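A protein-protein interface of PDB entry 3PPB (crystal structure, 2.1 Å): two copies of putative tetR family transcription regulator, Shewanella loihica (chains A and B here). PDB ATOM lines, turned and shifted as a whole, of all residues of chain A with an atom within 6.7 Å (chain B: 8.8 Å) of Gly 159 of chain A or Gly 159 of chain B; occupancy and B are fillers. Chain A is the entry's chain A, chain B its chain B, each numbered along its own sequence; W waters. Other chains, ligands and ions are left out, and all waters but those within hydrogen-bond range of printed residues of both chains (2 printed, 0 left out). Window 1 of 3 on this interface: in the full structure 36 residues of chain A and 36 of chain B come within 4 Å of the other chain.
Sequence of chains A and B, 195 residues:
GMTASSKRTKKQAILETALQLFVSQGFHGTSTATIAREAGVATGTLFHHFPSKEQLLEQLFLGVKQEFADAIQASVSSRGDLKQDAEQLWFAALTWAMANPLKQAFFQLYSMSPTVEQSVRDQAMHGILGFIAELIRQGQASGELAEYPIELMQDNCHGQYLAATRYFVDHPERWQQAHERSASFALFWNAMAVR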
ATOM      1  N   MET A 112      11.874 -19.620 -38.087  1.00  0.00           N
ATOM      2  CA  MET A 112      10.740 -20.423 -37.644  1.00  0.00           C
ATOM      3  C   MET A 112       9.540 -20.264 -38.560  1.00  0.00           C
ATOM      4  O   MET A 112       8.414 -20.647 -38.203  1.00  0.00           O
ATOM      5  CB  MET A 112      10.374 -19.994 -36.222  1.00  0.00           C
ATOM      6  CG  MET A 112      10.185 -21.168 -35.313  1.00  0.00           C
ATOM      7  SD  MET A 112      10.017 -20.623 -33.500  1.00  0.00           S
ATOM      8  CE  MET A 112       8.628 -19.382 -33.691  1.00  0.00           C
ATOM      9  N   GLN A 154      13.571 -27.646 -27.382  1.00  0.00           N
ATOM     10  CA  GLN A 154      14.484 -26.889 -28.261  1.00  0.00           C
ATOM     11  C   GLN A 154      13.702 -25.821 -29.016  1.00  0.00           C
ATOM     12  O   GLN A 154      14.197 -24.700 -29.112  1.00  0.00           O
ATOM     13  CB  GLN A 154      15.303 -27.765 -29.236  1.00  0.00           C
ATOM     14  CG  GLN A 154      16.450 -26.965 -29.895  1.00  0.00           C
ATOM     15  CD  GLN A 154      17.513 -27.743 -30.646  1.00  0.00           C
ATOM     16  OE1 GLN A 154      17.685 -28.959 -30.481  1.00  0.00           O
ATOM     17  NE2 GLN A 154      18.295 -27.032 -31.458  1.00  0.00           N
ATOM     18  N   ASP A 155      12.465 -26.121 -29.502  1.00  0.00           N
ATOM     19  CA  ASP A 155      11.651 -25.100 -30.180  1.00  0.00           C
ATOM     20  C   ASP A 155      11.364 -23.977 -29.214  1.00  0.00           C
ATOM     21  O   ASP A 155      11.352 -22.811 -29.608  1.00  0.00           O
ATOM     22  CB  ASP A 155      10.331 -25.676 -30.708  1.00  0.00           C
ATOM     23  CG  ASP A 155      10.447 -26.449 -32.007  1.00  0.00           C
ATOM     24  OD1 ASP A 155      11.535 -26.421 -32.618  1.00  0.00           O
ATOM     25  OD2 ASP A 155       9.451 -27.094 -32.400  1.00  0.00           O
ATOM     26  N   ASN A 156      11.114 -24.330 -27.938  1.00  0.00           N
ATOM     27  CA  ASN A 156      10.814 -23.343 -26.922  1.00  0.00           C
ATOM     28  C   ASN A 156      12.017 -22.423 -26.719  1.00  0.00           C
ATOM     29  O   ASN A 156      11.821 -21.210 -26.666  1.00  0.00           O
ATOM     30  CB  ASN A 156      10.365 -24.010 -25.626  1.00  0.00           C
ATOM     31  CG  ASN A 156      10.073 -23.005 -24.564  1.00  0.00           C
ATOM     32  OD1 ASN A 156       9.089 -22.249 -24.626  1.00  0.00           O
ATOM     33  ND2 ASN A 156      11.034 -22.879 -23.681  1.00  0.00           N
ATOM     34  N   CYS A 157      13.252 -22.979 -26.619  1.00  0.00           N
ATOM     35  CA  CYS A 157      14.483 -22.170 -26.499  1.00  0.00           C
ATOM     36  C   CYS A 157      14.550 -21.185 -27.655  1.00  0.00           C
ATOM     37  O   CYS A 157      14.839 -20.010 -27.464  1.00  0.00           O
ATOM     38  CB  CYS A 157      15.728 -23.057 -26.484  1.00  0.00           C
ATOM     39  SG  CYS A 157      15.876 -24.100 -25.031  1.00  0.00           S
ATOM     40  N   HIS A 158      14.273 -21.690 -28.863  1.00  0.00           N
ATOM     41  CA  HIS A 158      14.282 -20.933 -30.112  1.00  0.00           C
ATOM     42  C   HIS A 158      13.231 -19.805 -30.084  1.00  0.00           C
ATOM     43  O   HIS A 158      13.576 -18.661 -30.420  1.00  0.00           O
ATOM     44  CB  HIS A 158      14.040 -21.883 -31.281  1.00  0.00           C
ATOM     45  CG  HIS A 158      14.304 -21.323 -32.640  1.00  0.00           C
ATOM     46  ND1 HIS A 158      14.943 -20.118 -32.816  1.00  0.00           N
ATOM     47  CD2 HIS A 158      14.056 -21.864 -33.854  1.00  0.00           C
ATOM     48  CE1 HIS A 158      15.008 -19.940 -34.121  1.00  0.00           C
ATOM     49  NE2 HIS A 158      14.505 -20.975 -34.784  1.00  0.00           N
ATOM     50  N   GLY A 159      11.998 -20.110 -29.650  1.00  0.00           N
ATOM     51  CA  GLY A 159      10.942 -19.108 -29.547  1.00  0.00           C
ATOM     52  C   GLY A 159      11.260 -18.017 -28.529  1.00  0.00           C
ATOM     53  O   GLY A 159      10.969 -16.835 -28.760  1.00  0.00           O
ATOM     54  N   GLN A 160      11.847 -18.403 -27.387  1.00  0.00           N
ATOM     55  CA  GLN A 160      12.188 -17.442 -26.341  1.00  0.00           C
ATOM     56  C   GLN A 160      13.342 -16.575 -26.782  1.00  0.00           C
ATOM     57  O   GLN A 160      13.343 -15.384 -26.483  1.00  0.00           O
ATOM     58  CB  GLN A 160      12.494 -18.128 -25.010  1.00  0.00           C
ATOM     59  CG  GLN A 160      11.237 -18.774 -24.424  1.00  0.00           C
ATOM     60  CD  GLN A 160      11.467 -19.220 -23.028  1.00  0.00           C
ATOM     61  OE1 GLN A 160      12.120 -20.246 -22.785  1.00  0.00           O
ATOM     62  NE2 GLN A 160      10.952 -18.455 -22.077  1.00  0.00           N
ATOM     63  N   TYR A 161      14.304 -17.147 -27.527  1.00  0.00           N
ATOM     64  CA  TYR A 161      15.415 -16.355 -28.087  1.00  0.00           C
ATOM     65  C   TYR A 161      14.850 -15.295 -29.051  1.00  0.00           C
ATOM     66  O   TYR A 161      15.225 -14.119 -28.993  1.00  0.00           O
ATOM     67  CB  TYR A 161      16.426 -17.272 -28.809  1.00  0.00           C
ATOM     68  CG  TYR A 161      17.408 -16.515 -29.675  1.00  0.00           C
ATOM     69  CD1 TYR A 161      18.501 -15.854 -29.112  1.00  0.00           C
ATOM     70  CD2 TYR A 161      17.219 -16.408 -31.051  1.00  0.00           C
ATOM     71  CE1 TYR A 161      19.396 -15.125 -29.906  1.00  0.00           C
ATOM     72  CE2 TYR A 161      18.092 -15.657 -31.847  1.00  0.00           C
ATOM     73  CZ  TYR A 161      19.189 -15.032 -31.270  1.00  0.00           C
ATOM     74  OH  TYR A 161      20.070 -14.297 -32.029  1.00  0.00           O
ATOM     75  N   LEU A 162      13.945 -15.710 -29.940  1.00  0.00           N
ATOM     76  CA  LEU A 162      13.377 -14.782 -30.920  1.00  0.00           C
ATOM     77  C   LEU A 162      12.544 -13.708 -30.252  1.00  0.00           C
ATOM     78  O   LEU A 162      12.552 -12.569 -30.705  1.00  0.00           O
ATOM     79  CB  LEU A 162      12.566 -15.524 -31.991  1.00  0.00           C
ATOM     80  CG  LEU A 162      13.390 -16.414 -32.958  1.00  0.00           C
ATOM     81  CD1 LEU A 162      12.475 -17.212 -33.828  1.00  0.00           C
ATOM     82  CD2 LEU A 162      14.353 -15.578 -33.811  1.00  0.00           C
ATOM     83  N   ALA A 163      11.858 -14.049 -29.153  1.00  0.00           N
ATOM     84  CA  ALA A 163      11.051 -13.088 -28.398  1.00  0.00           C
ATOM     85  C   ALA A 163      11.958 -12.063 -27.705  1.00  0.00           C
ATOM     86  O   ALA A 163      11.674 -10.875 -27.764  1.00  0.00           O
ATOM     87  CB  ALA A 163      10.194 -13.811 -27.383  1.00  0.00           C
ATOM     88  N   ALA A 164      13.057 -12.518 -27.072  1.00  0.00           N
ATOM     89  CA  ALA A 164      13.964 -11.628 -26.329  1.00  0.00           C
ATOM     90  C   ALA A 164      14.731 -10.718 -27.280  1.00  0.00           C
ATOM     91  O   ALA A 164      14.922  -9.546 -26.962  1.00  0.00           O
ATOM     92  CB  ALA A 164      14.934 -12.437 -25.449  1.00  0.00           C
ATOM     93  N   TRP B  90      -4.297 -20.704 -23.233  1.00  0.00           N
ATOM     94  CA  TRP B  90      -3.195 -21.309 -23.952  1.00  0.00           C
ATOM     95  C   TRP B  90      -3.703 -22.418 -24.892  1.00  0.00           C
ATOM     96  O   TRP B  90      -3.356 -22.419 -26.069  1.00  0.00           O
ATOM     97  CB  TRP B  90      -2.199 -21.882 -22.936  1.00  0.00           C
ATOM     98  CG  TRP B  90      -1.090 -22.664 -23.562  1.00  0.00           C
ATOM     99  CD1 TRP B  90      -0.959 -24.014 -23.586  1.00  0.00           C
ATOM    100  CD2 TRP B  90       0.045 -22.136 -24.259  1.00  0.00           C
ATOM    101  NE1 TRP B  90       0.218 -24.361 -24.200  1.00  0.00           N
ATOM    102  CE2 TRP B  90       0.850 -23.229 -24.631  1.00  0.00           C
ATOM    103  CE3 TRP B  90       0.454 -20.831 -24.623  1.00  0.00           C
ATOM    104  CZ2 TRP B  90       2.064 -23.068 -25.315  1.00  0.00           C
ATOM    105  CZ3 TRP B  90       1.650 -20.672 -25.305  1.00  0.00           C
ATOM    106  CH2 TRP B  90       2.453 -21.783 -25.626  1.00  0.00           C
ATOM    107  N   GLN B 108       3.017 -16.717 -38.161  1.00  0.00           N
ATOM    108  CA  GLN B 108       4.407 -17.200 -38.206  1.00  0.00           C
ATOM    109  C   GLN B 108       5.260 -16.309 -39.113  1.00  0.00           C
ATOM    110  O   GLN B 108       6.393 -15.990 -38.760  1.00  0.00           O
ATOM    111  CB  GLN B 108       4.498 -18.674 -38.666  1.00  0.00           C
ATOM    112  CG  GLN B 108       4.109 -19.723 -37.588  1.00  0.00           C
ATOM    113  CD  GLN B 108       4.931 -19.771 -36.304  1.00  0.00           C
ATOM    114  OE1 GLN B 108       5.842 -18.977 -36.053  1.00  0.00           O
ATOM    115  NE2 GLN B 108       4.640 -20.747 -35.459  1.00  0.00           N
ATOM    116  N   SER B 111       3.801 -11.745 -37.465  1.00  0.00           N
ATOM    117  CA  SER B 111       3.576 -11.361 -36.050  1.00  0.00           C
ATOM    118  C   SER B 111       4.755 -10.732 -35.320  1.00  0.00           C
ATOM    119  O   SER B 111       4.543  -9.869 -34.453  1.00  0.00           O
ATOM    120  CB  SER B 111       3.152 -12.577 -35.234  1.00  0.00           C
ATOM    121  OG  SER B 111       1.752 -12.730 -35.340  1.00  0.00           O
ATOM    122  N   MET B 112       5.971 -11.223 -35.588  1.00  0.00           N
ATOM    123  CA  MET B 112       7.154 -10.764 -34.883  1.00  0.00           C
ATOM    124  C   MET B 112       8.259 -10.331 -35.829  1.00  0.00           C
ATOM    125  O   MET B 112       9.417 -10.162 -35.418  1.00  0.00           O
ATOM    126  CB  MET B 112       7.632 -11.902 -33.980  1.00  0.00           C
ATOM    127  CG  MET B 112       7.898 -11.443 -32.587  1.00  0.00           C
ATOM    128  SD  MET B 112       8.197 -12.888 -31.371  1.00  0.00           S
ATOM    129  CE  MET B 112       9.495 -13.823 -32.351  1.00  0.00           C
ATOM    130  N   LEU B 152       8.319  -7.470 -21.687  1.00  0.00           N
ATOM    131  CA  LEU B 152       9.231  -8.579 -21.964  1.00  0.00           C
ATOM    132  C   LEU B 152       8.458  -9.892 -21.773  1.00  0.00           C
ATOM    133  O   LEU B 152       8.592 -10.814 -22.559  1.00  0.00           O
ATOM    134  CB  LEU B 152      10.465  -8.503 -21.014  1.00  0.00           C
ATOM    135  CG  LEU B 152      11.469  -9.702 -21.100  1.00  0.00           C
ATOM    136  CD1 LEU B 152      11.959  -9.974 -22.550  1.00  0.00           C
ATOM    137  CD2 LEU B 152      12.630  -9.514 -20.163  1.00  0.00           C
ATOM    138  N   MET B 153       7.612  -9.952 -20.738  1.00  0.00           N
ATOM    139  CA  MET B 153       6.826 -11.146 -20.459  1.00  0.00           C
ATOM    140  C   MET B 153       5.811 -11.375 -21.540  1.00  0.00           C
ATOM    141  O   MET B 153       5.589 -12.521 -21.916  1.00  0.00           O
ATOM    142  CB  MET B 153       6.137 -11.033 -19.092  1.00  0.00           C
ATOM    143  CG  MET B 153       7.118 -10.940 -17.950  1.00  0.00           C
ATOM    144  SD  MET B 153       6.266 -10.826 -16.194  1.00  0.00           S
ATOM    145  CE  MET B 153       5.725 -12.626 -16.028  1.00  0.00           C
ATOM    146  N   GLN B 154       5.192 -10.302 -22.051  1.00  0.00           N
ATOM    147  CA  GLN B 154       4.201 -10.430 -23.112  1.00  0.00           C
ATOM    148  C   GLN B 154       4.889 -10.891 -24.431  1.00  0.00           C
ATOM    149  O   GLN B 154       4.379 -11.803 -25.086  1.00  0.00           O
ATOM    150  CB  GLN B 154       3.409  -9.127 -23.278  1.00  0.00           C
ATOM    151  CG  GLN B 154       2.251  -9.299 -24.263  1.00  0.00           C
ATOM    152  CD  GLN B 154       1.182  -8.235 -24.198  1.00  0.00           C
ATOM    153  OE1 GLN B 154       1.224  -7.286 -23.370  1.00  0.00           O
ATOM    154  NE2 GLN B 154       0.187  -8.401 -25.087  1.00  0.00           N
ATOM    155  N   ASP B 155       6.074 -10.343 -24.758  1.00  0.00           N
ATOM    156  CA  ASP B 155       6.833 -10.820 -25.944  1.00  0.00           C
ATOM    157  C   ASP B 155       7.201 -12.292 -25.762  1.00  0.00           C
ATOM    158  O   ASP B 155       7.144 -13.065 -26.705  1.00  0.00           O
ATOM    159  CB  ASP B 155       8.116  -9.998 -26.152  1.00  0.00           C
ATOM    160  CG  ASP B 155       7.908  -8.660 -26.846  1.00  0.00           C
ATOM    161  OD1 ASP B 155       6.772  -8.381 -27.275  1.00  0.00           O
ATOM    162  OD2 ASP B 155       8.862  -7.892 -26.927  1.00  0.00           O
ATOM    163  N   ASN B 156       7.555 -12.666 -24.516  1.00  0.00           N
ATOM    164  CA  ASN B 156       7.898 -14.041 -24.192  1.00  0.00           C
ATOM    165  C   ASN B 156       6.702 -14.954 -24.438  1.00  0.00           C
ATOM    166  O   ASN B 156       6.894 -16.002 -25.045  1.00  0.00           O
ATOM    167  CB  ASN B 156       8.402 -14.149 -22.750  1.00  0.00           C
ATOM    168  CG  ASN B 156       8.764 -15.556 -22.399  1.00  0.00           C
ATOM    169  OD1 ASN B 156       9.745 -16.137 -22.917  1.00  0.00           O
ATOM    170  ND2 ASN B 156       7.860 -16.179 -21.684  1.00  0.00           N
ATOM    171  N   CYS B 157       5.476 -14.567 -23.984  1.00  0.00           N
ATOM    172  CA  CYS B 157       4.233 -15.340 -24.225  1.00  0.00           C
ATOM    173  C   CYS B 157       4.085 -15.570 -25.717  1.00  0.00           C
ATOM    174  O   CYS B 157       3.795 -16.685 -26.148  1.00  0.00           O
ATOM    175  CB  CYS B 157       3.001 -14.629 -23.666  1.00  0.00           C
ATOM    176  SG  CYS B 157       2.955 -14.518 -21.860  1.00  0.00           S
ATOM    177  N   HIS B 158       4.282 -14.501 -26.491  1.00  0.00           N
ATOM    178  CA  HIS B 158       4.189 -14.489 -27.949  1.00  0.00           C
ATOM    179  C   HIS B 158       5.228 -15.442 -28.592  1.00  0.00           C
ATOM    180  O   HIS B 158       4.858 -16.239 -29.445  1.00  0.00           O
ATOM    181  CB  HIS B 158       4.383 -13.045 -28.448  1.00  0.00           C
ATOM    182  CG  HIS B 158       4.026 -12.824 -29.893  1.00  0.00           C
ATOM    183  ND1 HIS B 158       3.351 -13.779 -30.637  1.00  0.00           N
ATOM    184  CD2 HIS B 158       4.209 -11.726 -30.660  1.00  0.00           C
ATOM    185  CE1 HIS B 158       3.187 -13.246 -31.838  1.00  0.00           C
ATOM    186  NE2 HIS B 158       3.656 -12.001 -31.885  1.00  0.00           N
ATOM    187  N   GLY B 159       6.493 -15.370 -28.157  1.00  0.00           N
ATOM    188  CA  GLY B 159       7.527 -16.261 -28.668  1.00  0.00           C
ATOM    189  C   GLY B 159       7.258 -17.736 -28.345  1.00  0.00           C
ATOM    190  O   GLY B 159       7.502 -18.615 -29.175  1.00  0.00           O
ATOM    191  N   GLN B 160       6.759 -18.018 -27.131  1.00  0.00           N
ATOM    192  CA  GLN B 160       6.456 -19.392 -26.708  1.00  0.00           C
ATOM    193  C   GLN B 160       5.265 -19.931 -27.466  1.00  0.00           C
ATOM    194  O   GLN B 160       5.273 -21.103 -27.830  1.00  0.00           O
ATOM    195  CB  GLN B 160       6.247 -19.508 -25.210  1.00  0.00           C
ATOM    196  CG  GLN B 160       7.551 -19.249 -24.455  1.00  0.00           C
ATOM    197  CD  GLN B 160       7.403 -19.614 -23.010  1.00  0.00           C
ATOM    198  OE1 GLN B 160       6.778 -18.890 -22.240  1.00  0.00           O
ATOM    199  NE2 GLN B 160       7.952 -20.768 -22.631  1.00  0.00           N
ATOM    200  N   TYR B 161       4.276 -19.085 -27.745  1.00  0.00           N
ATOM    201  CA  TYR B 161       3.123 -19.493 -28.558  1.00  0.00           C
ATOM    202  C   TYR B 161       3.607 -19.869 -29.974  1.00  0.00           C
ATOM    203  O   TYR B 161       3.222 -20.893 -30.523  1.00  0.00           O
ATOM    204  CB  TYR B 161       2.083 -18.343 -28.632  1.00  0.00           C
ATOM    205  CG  TYR B 161       1.040 -18.550 -29.708  1.00  0.00           C
ATOM    206  CD1 TYR B 161      -0.039 -19.396 -29.501  1.00  0.00           C
ATOM    207  CD2 TYR B 161       1.152 -17.925 -30.950  1.00  0.00           C
ATOM    208  CE1 TYR B 161      -0.994 -19.618 -30.503  1.00  0.00           C
ATOM    209  CE2 TYR B 161       0.212 -18.155 -31.969  1.00  0.00           C
ATOM    210  CZ  TYR B 161      -0.870 -18.990 -31.728  1.00  0.00           C
ATOM    211  OH  TYR B 161      -1.814 -19.229 -32.705  1.00  0.00           O
ATOM    212  N   LEU B 162       4.464 -19.039 -30.559  1.00  0.00           N
ATOM    213  CA  LEU B 162       4.947 -19.302 -31.925  1.00  0.00           C
ATOM    214  C   LEU B 162       5.807 -20.560 -31.962  1.00  0.00           C
ATOM    215  O   LEU B 162       5.740 -21.316 -32.930  1.00  0.00           O
ATOM    216  CB  LEU B 162       5.688 -18.077 -32.509  1.00  0.00           C
ATOM    217  CG  LEU B 162       4.803 -16.831 -32.808  1.00  0.00           C
ATOM    218  CD1 LEU B 162       5.657 -15.662 -33.237  1.00  0.00           C
ATOM    219  CD2 LEU B 162       3.785 -17.100 -33.892  1.00  0.00           C
ATOM    220  N   ALA B 163       6.566 -20.818 -30.890  1.00  0.00           N
ATOM    221  CA  ALA B 163       7.397 -22.017 -30.800  1.00  0.00           C
ATOM    222  C   ALA B 163       6.516 -23.288 -30.694  1.00  0.00           C
ATOM    223  O   ALA B 163       6.783 -24.269 -31.383  1.00  0.00           O
ATOM    224  CB  ALA B 163       8.314 -21.919 -29.579  1.00  0.00           C
ATOM    225  N   ALA B 164       5.475 -23.256 -29.836  1.00  0.00           N
ATOM    226  CA  ALA B 164       4.594 -24.420 -29.610  1.00  0.00           C
ATOM    227  C   ALA B 164       3.756 -24.711 -30.841  1.00  0.00           C
ATOM    228  O   ALA B 164       3.552 -25.879 -31.152  1.00  0.00           O
ATOM    229  CB  ALA B 164       3.688 -24.199 -28.399  1.00  0.00           C
ATOM    230  N   THR B 165       3.298 -23.661 -31.546  1.00  0.00           N
ATOM    231  CA  THR B 165       2.476 -23.835 -32.752  1.00  0.00           C
ATOM    232  C   THR B 165       3.338 -24.280 -33.917  1.00  0.00           C
ATOM    233  O   THR B 165       2.833 -25.008 -34.745  1.00  0.00           O
ATOM    234  CB  THR B 165       1.622 -22.628 -33.072  1.00  0.00           C
ATOM    235  OG1 THR B 165       2.437 -21.471 -33.234  1.00  0.00           O
ATOM    236  CG2 THR B 165       0.572 -22.394 -32.026  1.00  0.00           C
ATOM    237  N   ARG B 166       4.626 -23.907 -33.963  1.00  0.00           N
ATOM    238  CA  ARG B 166       5.588 -24.382 -34.964  1.00  0.00           C
ATOM    239  C   ARG B 166       5.720 -25.884 -34.772  1.00  0.00           C
ATOM    240  O   ARG B 166       5.539 -26.646 -35.718  1.00  0.00           O
ATOM    241  CB  ARG B 166       6.966 -23.674 -34.790  1.00  0.00           C
ATOM    242  CG  ARG B 166       8.157 -24.298 -35.551  1.00  0.00           C
ATOM    243  CD  ARG B 166       8.197 -23.888 -37.027  1.00  0.00           C
ATOM    244  NE  ARG B 166       7.167 -24.577 -37.806  1.00  0.00           N
ATOM    245  CZ  ARG B 166       6.220 -23.980 -38.528  1.00  0.00           C
ATOM    246  NH1 ARG B 166       6.181 -22.657 -38.623  1.00  0.00           N
ATOM    247  NH2 ARG B 166       5.314 -24.704 -39.171  1.00  0.00           N
ATOM    248  N   PHE B 188       5.231 -22.825 -20.904  1.00  0.00           N
ATOM    249  CA  PHE B 188       4.619 -21.493 -20.940  1.00  0.00           C
ATOM    250  C   PHE B 188       4.427 -20.909 -19.500  1.00  0.00           C
ATOM    251  O   PHE B 188       4.874 -19.801 -19.223  1.00  0.00           O
ATOM    252  CB  PHE B 188       3.271 -21.574 -21.675  1.00  0.00           C
ATOM    253  CG  PHE B 188       2.469 -20.298 -21.664  1.00  0.00           C
ATOM    254  CD1 PHE B 188       2.847 -19.214 -22.449  1.00  0.00           C
ATOM    255  CD2 PHE B 188       1.319 -20.186 -20.887  1.00  0.00           C
ATOM    256  CE1 PHE B 188       2.087 -18.041 -22.463  1.00  0.00           C
ATOM    257  CE2 PHE B 188       0.568 -19.005 -20.890  1.00  0.00           C
ATOM    258  CZ  PHE B 188       0.963 -17.939 -21.671  1.00  0.00           C
HETATM  259  O   HOH W   1       7.079 -23.151 -26.308  1.00  0.00           O
HETATM  260  O   HOH W   2      11.799 -14.573 -24.080  1.00  0.00           O
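NH1 of Arg 166 of chain B is in hydrogen-bond range of O of Met 112 of chain A.
The side-chain amide nitrogen (NE2) of Gln 160 of chain B sits at hydrogen-bond distance from the side-chain amide oxygen (OD1) of Asn 156 of chain A.
OD1 of Asn 156 of chain B lies within hydrogen-bond range of NE2 of Gln 160 of chain A.
The side-chain amide nitrogen (ND2) of Asn 156 of chain B is in hydrogen-bond range of the side-chain amide oxygen (OE1) of Gln 160 of chain B (3.0 Å).
The side-chain amide nitrogen (NE2) of Gln 108 of chain B sits close to the backbone NH (N) of Arg 166 of chain B, 3.5 Å away.
The backbone carbonyl oxygen of Leu 162 of chain B lies within hydrogen-bond range of the side-chain hydroxyl of Thr 165 of chain B (3.3 Å).
The side-chain amide nitrogen (NE2) of Gln 108 of chain B is in hydrogen-bond range of the side-chain hydroxyl (OG1) of Thr 165 of chain B (3.2 Å).
The backbone carbonyl oxygen (O) of Leu 162 of chain B is in hydrogen-bond range of the side-chain amide nitrogen (NE2) of Gln 108 of chain B (2.8 Å).
OE1 of Gln 160 of chain A lies within hydrogen-bond range of ND2 of Asn 156 of chain A, at 3.0 Å.
Gln 108 of chain B touches Met 112 of chain A (OE1 to CE, 3.7 Å).
CE of Met 112 of chain A touches CB of Leu 162 of chain B (3.4 Å).
CE of Met 112 of chain A touches N of Ala 163 of chain B, at 3.8 Å.
Asn 156 of chain A touches Ala 163 of chain B (CA to CB, 3.9 Å).
Gly 159 of chain A touches Gly 159 of chain B.
Gln 160 of chain A touches Gln 160 of chain B (CG to CG, 3.7 Å).
Met 112 of chain B touches Leu 162 of chain A (CE to CB, 3.5 Å).
Met 112 of chain B touches Ala 163 of chain A.
CB of Ala 163 of chain A touches O of Asp 155 of chain B, at 3.2 Å.
Ala 163 of chain A touches Gly 159 of chain B (CB to CA, 3.8 Å).
Of the printed residues of chain B, Gly 159 of chain A touches Gly 159 (3.5 Å) and Ala 163 (3.8 Å).
Of chain A, only Gly 159 (3.5 Å) and Ala 163 (3.8 Å) come within 4 Å of Gly 159 of chain B.
Of the printed residues of chain A, Gln 160 of chain B touches Asn 156 and Gln 160.
Of the printed residues of chain A, Gln 108 of chain B touches Met 112.
Of the printed residues of chain B, Leu 162 of chain A touches Met 112 (3.5 Å).
Of the printed residues of chain A, Arg 166 of chain B touches Met 112.
His 158 of chain A touches none of the printed residues of chain B.
Gln 154 of chain A touches none of the printed residues of chain B.
The nearest printed residue of chain A that does not touch Gly 159 of chain B is Gln 160 of chain A (4.7 Å).
Of the 20 printed residues of chain B, 9 touch a printed residue of chain A.
Hydrophobic or aromatic side chains of chain B that line the printed part of chain A: Met 112, Leu 162 and Ala 163.
Along chain B the printed residues that touch a printed residue of chain A span positions 108 to 166.
Hydrophobic or aromatic side chains of chain A within 4 Å of the printed part of chain B: Met 112, Leu 162 and Ala 163.
Among the printed residues, no Asp or Glu carboxylate lies within 4 Å of a Lys or Arg side-chain nitrogen of the other chain.
Met 112 of chain A touches Ala 163 of chain B, and with the chains exchanged Ala 163 of chain A touches Met 112 of chain B.
Asn 156 of chain A touches Gln 160 of chain B, and with the chains exchanged Gln 160 of chain A touches Asn 156 of chain B.
Asn 156 of chain A touches Ala 163 of chain B, and with the chains exchanged Ala 163 of chain A touches Asn 156 of chain B.
Gly 159 of chain A touches Ala 163 of chain B, and with the chains exchanged Ala 163 of chain A touches Gly 159 of chain B.
Positions printed for both chains: 112, 154, 155, 156, 157, 158, 159, 160, 161, 162, 163 and 164.
Water W1 lies within hydrogen-bond range of OD1 of Asn 156 of chain A (2.8 Å) and O of Gln 160 of chain B (3.1 Å).
Water W2 bridges the side-chain amide oxygen of Asn 156 of chain B and the backbone carbonyl oxygen of Gln 160 of chain A.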
